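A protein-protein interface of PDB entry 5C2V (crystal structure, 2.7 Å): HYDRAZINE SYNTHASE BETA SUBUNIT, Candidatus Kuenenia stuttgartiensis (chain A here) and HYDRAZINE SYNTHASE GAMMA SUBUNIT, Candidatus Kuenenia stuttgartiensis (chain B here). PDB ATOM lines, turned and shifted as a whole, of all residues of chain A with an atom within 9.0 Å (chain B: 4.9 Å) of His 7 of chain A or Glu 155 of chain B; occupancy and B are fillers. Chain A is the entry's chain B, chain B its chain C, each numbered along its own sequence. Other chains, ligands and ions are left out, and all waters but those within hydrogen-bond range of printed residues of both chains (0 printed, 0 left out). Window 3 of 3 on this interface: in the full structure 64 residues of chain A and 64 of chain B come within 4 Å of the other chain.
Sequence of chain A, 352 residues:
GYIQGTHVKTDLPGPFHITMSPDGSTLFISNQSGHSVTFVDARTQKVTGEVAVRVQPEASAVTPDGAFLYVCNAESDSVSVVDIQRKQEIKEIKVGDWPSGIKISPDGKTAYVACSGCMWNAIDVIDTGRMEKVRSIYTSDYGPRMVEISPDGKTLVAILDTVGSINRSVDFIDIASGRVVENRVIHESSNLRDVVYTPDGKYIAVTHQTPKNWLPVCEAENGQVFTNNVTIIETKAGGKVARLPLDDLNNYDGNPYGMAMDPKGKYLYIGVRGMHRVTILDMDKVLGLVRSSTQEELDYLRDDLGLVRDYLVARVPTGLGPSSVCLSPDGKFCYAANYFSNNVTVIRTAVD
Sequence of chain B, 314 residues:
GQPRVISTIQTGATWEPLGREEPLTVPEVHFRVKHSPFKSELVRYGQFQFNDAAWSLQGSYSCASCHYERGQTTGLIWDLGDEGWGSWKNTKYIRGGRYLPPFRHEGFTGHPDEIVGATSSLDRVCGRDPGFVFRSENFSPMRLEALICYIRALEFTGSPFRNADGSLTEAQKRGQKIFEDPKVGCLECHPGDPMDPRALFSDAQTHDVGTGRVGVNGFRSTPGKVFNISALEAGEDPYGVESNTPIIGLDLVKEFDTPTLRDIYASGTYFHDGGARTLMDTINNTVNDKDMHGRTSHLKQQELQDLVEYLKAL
The side-chain amide nitrogen (NE2) of Gln 4 of chain A sits close to the guanidinium group (NH2) of Arg 95 of chain B (3.0 Å). O of Gly 5 of chain A lies within hydrogen-bond range of N of Glu 155 of chain B.
OH of Tyr 99 of chain B sits at hydrogen-bond distance from OE1 of Glu 155 of chain B (3.0 Å). OG1 of Thr 6 of chain A lies within hydrogen-bond range of O of Ile 3 of chain A, 2.5 Å away. N of Gly 96 of chain B lies within hydrogen-bond range of O of Leu 154 of chain B, at 2.9 Å. OG1 of Thr 6 of chain A sits close to N of Val 8 of chain A, at 3.4 Å. O of Glu 155 of chain B lies within hydrogen-bond range of NH1 of Arg 95 of chain B (2.5 Å). The guanidinium group (NH2) of Arg 98 of chain B is in salt-bridge range of the side-chain carboxylate (OE2) of Glu 155 of chain B (3.98 Å).
Among the printed residues, merely in contact across the chains: Thr 6 of chain A with Ala 153 of chain B (3.3 Å), His 7 of chain A with Glu 155 of chain B (3.5 Å), Gly 5 of chain A with Arg 95 of chain B (3.6 Å), Gly 5 of chain A with Leu 154 of chain B (3.7 Å) and Gly 5 of chain A with Ala 153 of chain B (3.7 Å).
His 7 of chain A touches just one residue of chain B: Glu 155. Of chain A, only Gly 5 (2.9 Å) and His 7 (3.5 Å) come within 4 Å of Glu 155 of chain B. Printed residues of chain B within 4 Å of Thr 6 of chain A: Ala 153 (3.3 Å). Printed residues of chain A within 4 Å of Leu 154 of chain B: Gly 5. Val 8 of chain A touches none of the printed residues of chain B. The nearest printed residue of chain A that does not touch Arg 95 of chain B is Thr 6 of chain A (5.6 Å).
Of the 10 printed residues of chain B, 4 touch a printed residue of chain A. Along chain B the printed residues that touch a printed residue of chain A span positions 95 to 155. Of the 11 printed residues of chain A, 4 touch a printed residue of chain B. Among the printed residues, 7 pairs touch across the chains.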
ATOM      1  N   GLY A   1      32.856 -16.643   9.774  1.00  0.00           N
ATOM      2  CA  GLY A   1      32.062 -16.399  10.963  1.00  0.00           C
ATOM      3  C   GLY A   1      30.848 -17.304  11.048  1.00  0.00           C
ATOM      4  O   GLY A   1      30.414 -17.865  10.043  1.00  0.00           O
ATOM      5  N   TYR A   2      30.294 -17.436  12.247  1.00  0.00           N
ATOM      6  CA  TYR A   2      29.178 -18.346  12.479  1.00  0.00           C
ATOM      7  C   TYR A   2      27.856 -17.615  12.679  1.00  0.00           C
ATOM      8  O   TYR A   2      27.810 -16.550  13.297  1.00  0.00           O
ATOM      9  CB  TYR A   2      29.460 -19.228  13.696  1.00  0.00           C
ATOM     10  CG  TYR A   2      30.650 -20.140  13.523  1.00  0.00           C
ATOM     11  CD1 TYR A   2      30.796 -20.909  12.378  1.00  0.00           C
ATOM     12  CD2 TYR A   2      31.634 -20.221  14.498  1.00  0.00           C
ATOM     13  CE1 TYR A   2      31.883 -21.742  12.213  1.00  0.00           C
ATOM     14  CE2 TYR A   2      32.727 -21.048  14.341  1.00  0.00           C
ATOM     15  CZ  TYR A   2      32.847 -21.806  13.197  1.00  0.00           C
ATOM     16  OH  TYR A   2      33.935 -22.633  13.037  1.00  0.00           O
ATOM     17  N   ILE A   3      26.784 -18.196  12.151  1.00  0.00           N
ATOM     18  CA  ILE A   3      25.441 -17.705  12.422  1.00  0.00           C
ATOM     19  C   ILE A   3      25.118 -17.976  13.884  1.00  0.00           C
ATOM     20  O   ILE A   3      25.403 -19.056  14.404  1.00  0.00           O
ATOM     21  CB  ILE A   3      24.390 -18.362  11.504  1.00  0.00           C
ATOM     22  CG1 ILE A   3      24.569 -17.874  10.066  1.00  0.00           C
ATOM     23  CG2 ILE A   3      22.977 -18.055  11.985  1.00  0.00           C
ATOM     24  CD1 ILE A   3      23.500 -18.360   9.116  1.00  0.00           C
ATOM     25  N   GLN A   4      24.530 -16.980  14.538  1.00  0.00           N
ATOM     26  CA  GLN A   4      24.308 -17.002  15.976  1.00  0.00           C
ATOM     27  C   GLN A   4      23.561 -18.253  16.454  1.00  0.00           C
ATOM     28  O   GLN A   4      22.512 -18.608  15.917  1.00  0.00           O
ATOM     29  CB  GLN A   4      23.545 -15.743  16.392  1.00  0.00           C
ATOM     30  CG  GLN A   4      23.203 -15.715  17.857  1.00  0.00           C
ATOM     31  CD  GLN A   4      21.800 -16.196  18.132  1.00  0.00           C
ATOM     32  OE1 GLN A   4      20.911 -16.083  17.286  1.00  0.00           O
ATOM     33  NE2 GLN A   4      21.609 -16.801  19.295  1.00  0.00           N
ATOM     34  N   GLY A   5      24.116 -18.916  17.468  1.00  0.00           N
ATOM     35  CA  GLY A   5      23.515 -20.111  18.036  1.00  0.00           C
ATOM     36  C   GLY A   5      23.761 -21.369  17.223  1.00  0.00           C
ATOM     37  O   GLY A   5      23.247 -22.440  17.549  1.00  0.00           O
ATOM     38  N   THR A   6      24.554 -21.242  16.162  1.00  0.00           N
ATOM     39  CA  THR A   6      24.805 -22.358  15.255  1.00  0.00           C
ATOM     40  C   THR A   6      26.294 -22.602  15.024  1.00  0.00           C
ATOM     41  O   THR A   6      27.130 -21.743  15.306  1.00  0.00           O
ATOM     42  CB  THR A   6      24.147 -22.131  13.882  1.00  0.00           C
ATOM     43  OG1 THR A   6      24.896 -21.152  13.150  1.00  0.00           O
ATOM     44  CG2 THR A   6      22.708 -21.658  14.037  1.00  0.00           C
ATOM     45  N   HIS A   7      26.613 -23.787  14.517  1.00  0.00           N
ATOM     46  CA  HIS A   7      27.973 -24.109  14.099  1.00  0.00           C
ATOM     47  C   HIS A   7      28.160 -23.900  12.595  1.00  0.00           C
ATOM     48  O   HIS A   7      29.232 -24.170  12.053  1.00  0.00           O
ATOM     49  CB  HIS A   7      28.327 -25.543  14.495  1.00  0.00           C
ATOM     50  CG  HIS A   7      28.436 -25.745  15.974  1.00  0.00           C
ATOM     51  ND1 HIS A   7      29.315 -25.035  16.758  1.00  0.00           N
ATOM     52  CD2 HIS A   7      27.768 -26.573  16.814  1.00  0.00           C
ATOM     53  CE1 HIS A   7      29.191 -25.414  18.017  1.00  0.00           C
ATOM     54  NE2 HIS A   7      28.256 -26.350  18.076  1.00  0.00           N
ATOM     55  N   VAL A   8      27.112 -23.427  11.928  1.00  0.00           N
ATOM     56  CA  VAL A   8      27.167 -23.165  10.491  1.00  0.00           C
ATOM     57  C   VAL A   8      27.921 -21.871  10.188  1.00  0.00           C
ATOM     58  O   VAL A   8      27.659 -20.833  10.794  1.00  0.00           O
ATOM     59  CB  VAL A   8      25.756 -23.079   9.878  1.00  0.00           C
ATOM     60  CG1 VAL A   8      25.844 -22.972   8.363  1.00  0.00           C
ATOM     61  CG2 VAL A   8      24.927 -24.289  10.280  1.00  0.00           C
ATOM     62  N   LYS A   9      28.856 -21.943   9.245  1.00  0.00           N
ATOM     63  CA  LYS A   9      29.691 -20.799   8.887  1.00  0.00           C
ATOM     64  C   LYS A   9      29.089 -19.910   7.799  1.00  0.00           C
ATOM     65  O   LYS A   9      28.442 -20.392   6.870  1.00  0.00           O
ATOM     66  CB  LYS A   9      31.074 -21.279   8.444  1.00  0.00           C
ATOM     67  CG  LYS A   9      32.172 -20.260   8.687  1.00  0.00           C
ATOM     68  CD  LYS A   9      33.542 -20.834   8.388  1.00  0.00           C
ATOM     69  CE  LYS A   9      34.192 -21.352   9.656  1.00  0.00           C
ATOM     70  NZ  LYS A   9      35.593 -21.775   9.425  1.00  0.00           N
ATOM     71  N   THR A  10      29.310 -18.604   7.931  1.00  0.00           N
ATOM     72  CA  THR A  10      28.900 -17.637   6.917  1.00  0.00           C
ATOM     73  C   THR A  10      30.001 -16.606   6.673  1.00  0.00           C
ATOM     74  O   THR A  10      30.781 -16.292   7.572  1.00  0.00           O
ATOM     75  CB  THR A  10      27.601 -16.910   7.317  1.00  0.00           C
ATOM     76  OG1 THR A  10      27.273 -15.932   6.321  1.00  0.00           O
ATOM     77  CG2 THR A  10      27.764 -16.220   8.664  1.00  0.00           C
ATOM     78  N   GLU A  75      28.762 -13.957  23.035  1.00  0.00           N
ATOM     79  CA  GLU A  75      29.057 -15.376  23.178  1.00  0.00           C
ATOM     80  C   GLU A  75      30.294 -15.587  24.041  1.00  0.00           C
ATOM     81  O   GLU A  75      30.372 -16.543  24.813  1.00  0.00           O
ATOM     82  CB  GLU A  75      29.247 -16.031  21.810  1.00  0.00           C
ATOM     83  CG  GLU A  75      29.512 -17.527  21.869  1.00  0.00           C
ATOM     84  CD  GLU A  75      28.381 -18.295  22.530  1.00  0.00           C
ATOM     85  OE1 GLU A  75      27.472 -18.755  21.807  1.00  0.00           O
ATOM     86  OE2 GLU A  75      28.403 -18.446  23.770  1.00  0.00           O
ATOM     87  N   ARG B  95      16.379 -24.321  21.176  1.00  0.00           N
ATOM     88  CA  ARG B  95      17.777 -24.737  21.064  1.00  0.00           C
ATOM     89  C   ARG B  95      17.878 -26.258  21.133  1.00  0.00           C
ATOM     90  O   ARG B  95      17.250 -26.888  21.986  1.00  0.00           O
ATOM     91  CB  ARG B  95      18.641 -24.109  22.159  1.00  0.00           C
ATOM     92  CG  ARG B  95      18.835 -22.606  22.048  1.00  0.00           C
ATOM     93  CD  ARG B  95      19.510 -22.221  20.742  1.00  0.00           C
ATOM     94  NE  ARG B  95      20.010 -20.849  20.774  1.00  0.00           N
ATOM     95  CZ  ARG B  95      21.278 -20.522  21.006  1.00  0.00           C
ATOM     96  NH1 ARG B  95      22.183 -21.468  21.213  1.00  0.00           N
ATOM     97  NH2 ARG B  95      21.645 -19.248  21.020  1.00  0.00           N
ATOM     98  N   GLY B  96      18.667 -26.840  20.234  1.00  0.00           N
ATOM     99  CA  GLY B  96      18.859 -28.280  20.197  1.00  0.00           C
ATOM    100  C   GLY B  96      17.570 -29.044  19.959  1.00  0.00           C
ATOM    101  O   GLY B  96      17.273 -30.012  20.658  1.00  0.00           O
ATOM    102  N   ARG B  98      16.502 -30.698  17.091  1.00  0.00           N
ATOM    103  CA  ARG B  98      16.544 -31.880  16.234  1.00  0.00           C
ATOM    104  C   ARG B  98      16.929 -33.147  16.994  1.00  0.00           C
ATOM    105  O   ARG B  98      16.657 -34.258  16.539  1.00  0.00           O
ATOM    106  CB  ARG B  98      17.519 -31.662  15.073  1.00  0.00           C
ATOM    107  CG  ARG B  98      18.983 -31.593  15.483  1.00  0.00           C
ATOM    108  CD  ARG B  98      19.897 -31.607  14.266  1.00  0.00           C
ATOM    109  NE  ARG B  98      21.308 -31.637  14.643  1.00  0.00           N
ATOM    110  CZ  ARG B  98      22.312 -31.751  13.780  1.00  0.00           C
ATOM    111  NH1 ARG B  98      22.065 -31.849  12.480  1.00  0.00           N
ATOM    112  NH2 ARG B  98      23.564 -31.771  14.215  1.00  0.00           N
ATOM    113  N   TYR B  99      17.558 -32.977  18.151  1.00  0.00           N
ATOM    114  CA  TYR B  99      18.094 -34.108  18.900  1.00  0.00           C
ATOM    115  C   TYR B  99      17.022 -34.911  19.631  1.00  0.00           C
ATOM    116  O   TYR B  99      17.265 -36.050  20.031  1.00  0.00           O
ATOM    117  CB  TYR B  99      19.145 -33.625  19.902  1.00  0.00           C
ATOM    118  CG  TYR B  99      20.365 -33.015  19.254  1.00  0.00           C
ATOM    119  CD1 TYR B  99      20.845 -33.500  18.044  1.00  0.00           C
ATOM    120  CD2 TYR B  99      21.035 -31.954  19.846  1.00  0.00           C
ATOM    121  CE1 TYR B  99      21.959 -32.947  17.445  1.00  0.00           C
ATOM    122  CE2 TYR B  99      22.150 -31.393  19.253  1.00  0.00           C
ATOM    123  CZ  TYR B  99      22.607 -31.894  18.053  1.00  0.00           C
ATOM    124  OH  TYR B  99      23.717 -31.340  17.458  1.00  0.00           O
ATOM    125  N   ARG B 152      16.947 -26.760  12.972  1.00  0.00           N
ATOM    126  CA  ARG B 152      17.781 -27.926  13.245  1.00  0.00           C
ATOM    127  C   ARG B 152      19.224 -27.533  13.553  1.00  0.00           C
ATOM    128  O   ARG B 152      19.943 -28.264  14.233  1.00  0.00           O
ATOM    129  CB  ARG B 152      17.745 -28.892  12.058  1.00  0.00           C
ATOM    130  CG  ARG B 152      16.398 -29.566  11.855  1.00  0.00           C
ATOM    131  CD  ARG B 152      16.283 -30.203  10.478  1.00  0.00           C
ATOM    132  NE  ARG B 152      17.227 -31.299  10.285  1.00  0.00           N
ATOM    133  CZ  ARG B 152      17.271 -32.057   9.194  1.00  0.00           C
ATOM    134  NH1 ARG B 152      16.421 -31.838   8.198  1.00  0.00           N
ATOM    135  NH2 ARG B 152      18.161 -33.036   9.096  1.00  0.00           N
ATOM    136  N   ALA B 153      19.638 -26.373  13.054  1.00  0.00           N
ATOM    137  CA  ALA B 153      21.015 -25.918  13.205  1.00  0.00           C
ATOM    138  C   ALA B 153      21.248 -25.219  14.541  1.00  0.00           C
ATOM    139  O   ALA B 153      22.366 -24.800  14.842  1.00  0.00           O
ATOM    140  CB  ALA B 153      21.390 -24.994  12.058  1.00  0.00           C
ATOM    141  N   LEU B 154      20.193 -25.094  15.339  1.00  0.00           N
ATOM    142  CA  LEU B 154      20.300 -24.451  16.644  1.00  0.00           C
ATOM    143  C   LEU B 154      20.885 -25.399  17.686  1.00  0.00           C
ATOM    144  O   LEU B 154      20.399 -26.515  17.871  1.00  0.00           O
ATOM    145  CB  LEU B 154      18.935 -23.936  17.102  1.00  0.00           C
ATOM    146  CG  LEU B 154      18.396 -22.727  16.334  1.00  0.00           C
ATOM    147  CD1 LEU B 154      17.009 -22.344  16.827  1.00  0.00           C
ATOM    148  CD2 LEU B 154      19.356 -21.551  16.448  1.00  0.00           C
ATOM    149  N   GLU B 155      21.931 -24.940  18.367  1.00  0.00           N
ATOM    150  CA  GLU B 155      22.633 -25.748  19.358  1.00  0.00           C
ATOM    151  C   GLU B 155      22.495 -25.149  20.752  1.00  0.00           C
ATOM    152  O   GLU B 155      22.252 -23.951  20.898  1.00  0.00           O
ATOM    153  CB  GLU B 155      24.114 -25.878  18.992  1.00  0.00           C
ATOM    154  CG  GLU B 155      24.377 -26.460  17.611  1.00  0.00           C
ATOM    155  CD  GLU B 155      24.115 -27.952  17.541  1.00  0.00           C
ATOM    156  OE1 GLU B 155      24.026 -28.595  18.608  1.00  0.00           O
ATOM    157  OE2 GLU B 155      24.003 -28.484  16.416  1.00  0.00           O
ATOM    158  N   PHE B 156      22.644 -25.989  21.773  1.00  0.00           N
ATOM    159  CA  PHE B 156      22.553 -25.539  23.159  1.00  0.00           C
ATOM    160  C   PHE B 156      23.621 -24.500  23.497  1.00  0.00           C
ATOM    161  O   PHE B 156      24.725 -24.529  22.954  1.00  0.00           O
ATOM    162  CB  PHE B 156      22.664 -26.727  24.117  1.00  0.00           C
ATOM    163  CG  PHE B 156      21.540 -27.718  23.996  1.00  0.00           C
ATOM    164  CD1 PHE B 156      20.259 -27.388  24.406  1.00  0.00           C
ATOM    165  CD2 PHE B 156      21.767 -28.985  23.484  1.00  0.00           C
ATOM    166  CE1 PHE B 156      19.223 -28.299  24.298  1.00  0.00           C
ATOM    167  CE2 PHE B 156      20.738 -29.900  23.374  1.00  0.00           C
ATOM    168  CZ  PHE B 156      19.464 -29.558  23.782  1.00  0.00           C
ATOM    169  N   THR B 157      23.277 -23.580  24.394  1.00  0.00           N
ATOM    170  CA  THR B 157      24.202 -22.534  24.820  1.00  0.00           C
ATOM    171  C   THR B 157      25.200 -23.037  25.857  1.00  0.00           C
ATOM    172  O   THR B 157      26.359 -22.626  25.867  1.00  0.00           O
ATOM    173  CB  THR B 157      23.452 -21.324  25.414  1.00  0.00           C
ATOM    174  OG1 THR B 157      22.711 -21.738  26.569  1.00  0.00           O
ATOM    175  CG2 THR B 157      22.500 -20.728  24.392  1.00  0.00           C
